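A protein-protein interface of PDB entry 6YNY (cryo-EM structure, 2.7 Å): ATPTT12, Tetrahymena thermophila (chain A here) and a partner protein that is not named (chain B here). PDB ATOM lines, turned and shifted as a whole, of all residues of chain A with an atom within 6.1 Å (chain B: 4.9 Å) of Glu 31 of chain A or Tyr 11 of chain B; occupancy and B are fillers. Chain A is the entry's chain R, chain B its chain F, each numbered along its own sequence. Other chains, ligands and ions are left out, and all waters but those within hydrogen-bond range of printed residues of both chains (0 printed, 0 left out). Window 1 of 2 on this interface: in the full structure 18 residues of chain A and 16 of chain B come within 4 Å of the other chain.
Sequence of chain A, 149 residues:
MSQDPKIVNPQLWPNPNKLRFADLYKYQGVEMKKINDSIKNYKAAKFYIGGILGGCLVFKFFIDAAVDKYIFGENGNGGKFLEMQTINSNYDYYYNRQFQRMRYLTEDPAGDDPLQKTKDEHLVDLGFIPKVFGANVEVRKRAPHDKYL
The side-chain carboxylate (OE2) of Glu 31 of chain A sits at hydrogen-bond distance from the side-chain amide nitrogen (NE2) of Gln 8 of chain B, at 3.5 Å.
Gln 8 of chain B touches Val 30 of chain A (OE1 to CG2, 3.7 Å).
CE2 of Tyr 11 of chain B touches OE2 of Glu 31 of chain A, at 3.6 Å.
Of the printed residues of chain B, Val 30 of chain A touches Gln 8.
Printed residues of chain B within 4 Å of Glu 31 of chain A: Gln 8 and Tyr 11.
Printed residues of chain A within 4 Å of Gln 8 of chain B: Val 30 and Glu 31.
Asp 10 of chain B touches none of the printed residues of chain A.
Of the printed residues of chain A, Tyr 11 of chain B touches Glu 31.
The nearest printed residue of chain B that does not touch Glu 31 of chain A is Leu 12 of chain B (6.2 Å).
The nearest printed residue of chain A that does not touch Tyr 11 of chain B is Val 30 of chain A (7.6 Å).
Of the 9 printed residues of chain A, 2 touch a printed residue of chain B.
Printed residues of chain A that touch a printed residue of chain B: Val 30 and Glu 31.
Hydrophobic or aromatic side chains of chain A within 4 Å of the printed part of chain B: Val 30.
Along chain A the printed residues that touch a printed residue of chain B span positions 30 to 31.
Among the printed residues, 3 pairs touch across the chains.
Among the printed residues, no Asp or Glu carboxylate lies within 4 Å of a Lys or Arg side-chain nitrogen of the other chain.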
ATOM      1  N   GLN A  28     -12.461   0.188  -7.529  1.00  0.00           N
ATOM      2  CA  GLN A  28     -11.129   0.234  -6.923  1.00  0.00           C
ATOM      3  C   GLN A  28     -10.174  -0.760  -7.590  1.00  0.00           C
ATOM      4  O   GLN A  28      -9.699  -1.715  -6.974  1.00  0.00           O
ATOM      5  CB  GLN A  28     -11.207  -0.018  -5.415  1.00  0.00           C
ATOM      6  CG  GLN A  28     -11.931   1.062  -4.637  1.00  0.00           C
ATOM      7  CD  GLN A  28     -11.191   2.381  -4.650  1.00  0.00           C
ATOM      8  OE1 GLN A  28      -9.985   2.426  -4.887  1.00  0.00           O
ATOM      9  NE2 GLN A  28     -11.912   3.467  -4.395  1.00  0.00           N
ATOM     10  N   GLY A  29      -9.901  -0.526  -8.868  1.00  0.00           N
ATOM     11  CA  GLY A  29      -9.022  -1.378  -9.642  1.00  0.00           C
ATOM     12  C   GLY A  29      -7.565  -0.978  -9.552  1.00  0.00           C
ATOM     13  O   GLY A  29      -7.143  -0.243  -8.657  1.00  0.00           O
ATOM     14  N   VAL A  30      -6.784  -1.480 -10.511  1.00  0.00           N
ATOM     15  CA  VAL A  30      -5.348  -1.225 -10.508  1.00  0.00           C
ATOM     16  C   VAL A  30      -5.063   0.252 -10.721  1.00  0.00           C
ATOM     17  O   VAL A  30      -4.051   0.773 -10.238  1.00  0.00           O
ATOM     18  CB  VAL A  30      -4.639  -2.087 -11.570  1.00  0.00           C
ATOM     19  CG1 VAL A  30      -4.821  -3.561 -11.277  1.00  0.00           C
ATOM     20  CG2 VAL A  30      -5.144  -1.762 -12.953  1.00  0.00           C
ATOM     21  N   GLU A  31      -5.933   0.947 -11.450  1.00  0.00           N
ATOM     22  CA  GLU A  31      -5.745   2.376 -11.667  1.00  0.00           C
ATOM     23  C   GLU A  31      -5.765   3.133 -10.347  1.00  0.00           C
ATOM     24  O   GLU A  31      -4.915   3.993 -10.096  1.00  0.00           O
ATOM     25  CB  GLU A  31      -6.827   2.900 -12.605  1.00  0.00           C
ATOM     26  CG  GLU A  31      -6.406   4.082 -13.443  1.00  0.00           C
ATOM     27  CD  GLU A  31      -5.481   3.683 -14.576  1.00  0.00           C
ATOM     28  OE1 GLU A  31      -4.394   4.280 -14.703  1.00  0.00           O
ATOM     29  OE2 GLU A  31      -5.842   2.764 -15.340  1.00  0.00           O
ATOM     30  N   MET A  32      -6.739   2.826  -9.489  1.00  0.00           N
ATOM     31  CA  MET A  32      -6.812   3.482  -8.190  1.00  0.00           C
ATOM     32  C   MET A  32      -5.657   3.074  -7.291  1.00  0.00           C
ATOM     33  O   MET A  32      -5.182   3.884  -6.488  1.00  0.00           O
ATOM     34  CB  MET A  32      -8.140   3.157  -7.513  1.00  0.00           C
ATOM     35  CG  MET A  32      -9.343   3.826  -8.149  1.00  0.00           C
ATOM     36  SD  MET A  32      -9.236   5.621  -8.156  1.00  0.00           S
ATOM     37  CE  MET A  32      -9.118   5.961  -6.407  1.00  0.00           C
ATOM     38  N   LYS A  33      -5.198   1.828  -7.401  1.00  0.00           N
ATOM     39  CA  LYS A  33      -4.090   1.379  -6.569  1.00  0.00           C
ATOM     40  C   LYS A  33      -2.846   2.215  -6.830  1.00  0.00           C
ATOM     41  O   LYS A  33      -2.091   2.527  -5.904  1.00  0.00           O
ATOM     42  CB  LYS A  33      -3.812  -0.098  -6.824  1.00  0.00           C
ATOM     43  CG  LYS A  33      -2.970  -0.754  -5.754  1.00  0.00           C
ATOM     44  CD  LYS A  33      -2.623  -2.180  -6.120  1.00  0.00           C
ATOM     45  CE  LYS A  33      -1.779  -2.841  -5.040  1.00  0.00           C
ATOM     46  NZ  LYS A  33      -0.505  -2.109  -4.808  1.00  0.00           N
ATOM     47  N   LYS A  34      -2.614   2.582  -8.090  1.00  0.00           N
ATOM     48  CA  LYS A  34      -1.518   3.487  -8.412  1.00  0.00           C
ATOM     49  C   LYS A  34      -1.731   4.848  -7.768  1.00  0.00           C
ATOM     50  O   LYS A  34      -0.808   5.430  -7.189  1.00  0.00           O
ATOM     51  CB  LYS A  34      -1.398   3.646  -9.924  1.00  0.00           C
ATOM     52  CG  LYS A  34      -1.166   2.380 -10.694  1.00  0.00           C
ATOM     53  CD  LYS A  34      -1.252   2.669 -12.174  1.00  0.00           C
ATOM     54  CE  LYS A  34      -0.953   1.464 -13.016  1.00  0.00           C
ATOM     55  NZ  LYS A  34      -1.171   1.781 -14.450  1.00  0.00           N
ATOM     56  N   ILE A  35      -2.950   5.376  -7.874  1.00  0.00           N
ATOM     57  CA  ILE A  35      -3.235   6.708  -7.351  1.00  0.00           C
ATOM     58  C   ILE A  35      -3.058   6.734  -5.842  1.00  0.00           C
ATOM     59  O   ILE A  35      -2.512   7.692  -5.282  1.00  0.00           O
ATOM     60  CB  ILE A  35      -4.652   7.140  -7.770  1.00  0.00           C
ATOM     61  CG1 ILE A  35      -4.733   7.239  -9.293  1.00  0.00           C
ATOM     62  CG2 ILE A  35      -5.018   8.457  -7.130  1.00  0.00           C
ATOM     63  CD1 ILE A  35      -6.123   7.303  -9.833  1.00  0.00           C
ATOM     64  N   ASN A  36      -3.507   5.682  -5.158  1.00  0.00           N
ATOM     65  CA  ASN A  36      -3.350   5.627  -3.712  1.00  0.00           C
ATOM     66  C   ASN A  36      -1.882   5.597  -3.313  1.00  0.00           C
ATOM     67  O   ASN A  36      -1.523   6.075  -2.231  1.00  0.00           O
ATOM     68  CB  ASN A  36      -4.089   4.415  -3.152  1.00  0.00           C
ATOM     69  CG  ASN A  36      -5.586   4.523  -3.318  1.00  0.00           C
ATOM     70  OD1 ASN A  36      -6.131   5.617  -3.446  1.00  0.00           O
ATOM     71  ND2 ASN A  36      -6.263   3.385  -3.311  1.00  0.00           N
ATOM     72  N   MET B   7     -12.001  -5.557 -16.989  1.00  0.00           N
ATOM     73  CA  MET B   7     -12.226  -4.137 -16.755  1.00  0.00           C
ATOM     74  C   MET B   7     -11.077  -3.303 -17.299  1.00  0.00           C
ATOM     75  O   MET B   7     -11.289  -2.199 -17.811  1.00  0.00           O
ATOM     76  CB  MET B   7     -12.415  -3.880 -15.263  1.00  0.00           C
ATOM     77  CG  MET B   7     -13.653  -4.532 -14.682  1.00  0.00           C
ATOM     78  SD  MET B   7     -15.184  -3.888 -15.369  1.00  0.00           S
ATOM     79  CE  MET B   7     -15.131  -2.218 -14.747  1.00  0.00           C
ATOM     80  N   GLN B   8      -9.853  -3.816 -17.202  1.00  0.00           N
ATOM     81  CA  GLN B   8      -8.697  -3.057 -17.654  1.00  0.00           C
ATOM     82  C   GLN B   8      -8.557  -3.114 -19.169  1.00  0.00           C
ATOM     83  O   GLN B   8      -8.308  -2.089 -19.810  1.00  0.00           O
ATOM     84  CB  GLN B   8      -7.435  -3.583 -16.973  1.00  0.00           C
ATOM     85  CG  GLN B   8      -6.227  -2.692 -17.110  1.00  0.00           C
ATOM     86  CD  GLN B   8      -6.423  -1.337 -16.471  1.00  0.00           C
ATOM     87  OE1 GLN B   8      -7.398  -1.106 -15.761  1.00  0.00           O
ATOM     88  NE2 GLN B   8      -5.492  -0.433 -16.716  1.00  0.00           N
ATOM     89  N   THR B   9      -8.718  -4.300 -19.756  1.00  0.00           N
ATOM     90  CA  THR B   9      -8.539  -4.440 -21.196  1.00  0.00           C
ATOM     91  C   THR B   9      -9.527  -3.570 -21.962  1.00  0.00           C
ATOM     92  O   THR B   9      -9.181  -2.985 -22.994  1.00  0.00           O
ATOM     93  CB  THR B   9      -8.679  -5.905 -21.604  1.00  0.00           C
ATOM     94  OG1 THR B   9      -9.879  -6.452 -21.048  1.00  0.00           O
ATOM     95  CG2 THR B   9      -7.493  -6.700 -21.113  1.00  0.00           C
ATOM     96  N   ASP B  10     -10.766  -3.479 -21.477  1.00  0.00           N
ATOM     97  CA  ASP B  10     -11.740  -2.596 -22.104  1.00  0.00           C
ATOM     98  C   ASP B  10     -11.348  -1.134 -21.943  1.00  0.00           C
ATOM     99  O   ASP B  10     -11.704  -0.300 -22.781  1.00  0.00           O
ATOM    100  CB  ASP B  10     -13.123  -2.856 -21.514  1.00  0.00           C
ATOM    101  CG  ASP B  10     -14.181  -1.920 -22.054  1.00  0.00           C
ATOM    102  OD1 ASP B  10     -14.123  -0.710 -21.751  1.00  0.00           O
ATOM    103  OD2 ASP B  10     -15.071  -2.393 -22.790  1.00  0.00           O
ATOM    104  N   TYR B  11     -10.615  -0.811 -20.880  1.00  0.00           N
ATOM    105  CA  TYR B  11     -10.219   0.566 -20.621  1.00  0.00           C
ATOM    106  C   TYR B  11      -9.080   1.008 -21.532  1.00  0.00           C
ATOM    107  O   TYR B  11      -8.947   2.203 -21.812  1.00  0.00           O
ATOM    108  CB  TYR B  11      -9.825   0.705 -19.149  1.00  0.00           C
ATOM    109  CG  TYR B  11      -9.608   2.114 -18.656  1.00  0.00           C
ATOM    110  CD1 TYR B  11     -10.671   2.985 -18.482  1.00  0.00           C
ATOM    111  CD2 TYR B  11      -8.341   2.561 -18.325  1.00  0.00           C
ATOM    112  CE1 TYR B  11     -10.472   4.269 -18.017  1.00  0.00           C
ATOM    113  CE2 TYR B  11      -8.133   3.837 -17.861  1.00  0.00           C
ATOM    114  CZ  TYR B  11      -9.200   4.687 -17.705  1.00  0.00           C
ATOM    115  OH  TYR B  11      -8.984   5.963 -17.240  1.00  0.00           O
ATOM    116  N   LEU B  12      -8.260   0.069 -22.004  1.00  0.00           N
ATOM    117  CA  LEU B  12      -7.073   0.413 -22.776  1.00  0.00           C
ATOM    118  C   LEU B  12      -7.341   0.550 -24.266  1.00  0.00           C
ATOM    119  O   LEU B  12      -6.676   1.351 -24.929  1.00  0.00           O
ATOM    120  CB  LEU B  12      -5.979  -0.641 -22.585  1.00  0.00           C
ATOM    121  CG  LEU B  12      -5.022  -0.541 -21.394  1.00  0.00           C
ATOM    122  CD1 LEU B  12      -4.544   0.873 -21.144  1.00  0.00           C
ATOM    123  CD2 LEU B  12      -5.659  -1.092 -20.167  1.00  0.00           C
ATOM    124  N   TRP B  13      -8.272  -0.226 -24.813  1.00  0.00           N
ATOM    125  CA  TRP B  13      -8.417  -0.346 -26.254  1.00  0.00           C
ATOM    126  C   TRP B  13      -9.891  -0.377 -26.633  1.00  0.00           C
ATOM    127  O   TRP B  13     -10.770  -0.575 -25.791  1.00  0.00           O
ATOM    128  CB  TRP B  13      -7.687  -1.594 -26.763  1.00  0.00           C
ATOM    129  CG  TRP B  13      -7.494  -1.628 -28.237  1.00  0.00           C
ATOM    130  CD1 TRP B  13      -7.846  -2.633 -29.079  1.00  0.00           C
ATOM    131  CD2 TRP B  13      -6.909  -0.609 -29.049  1.00  0.00           C
ATOM    132  NE1 TRP B  13      -7.516  -2.307 -30.368  1.00  0.00           N
ATOM    133  CE2 TRP B  13      -6.939  -1.068 -30.377  1.00  0.00           C
ATOM    134  CE3 TRP B  13      -6.363   0.649 -28.784  1.00  0.00           C
ATOM    135  CZ2 TRP B  13      -6.445  -0.317 -31.434  1.00  0.00           C
ATOM    136  CZ3 TRP B  13      -5.874   1.388 -29.833  1.00  0.00           C
ATOM    137  CH2 TRP B  13      -5.917   0.907 -31.142  1.00  0.00           C
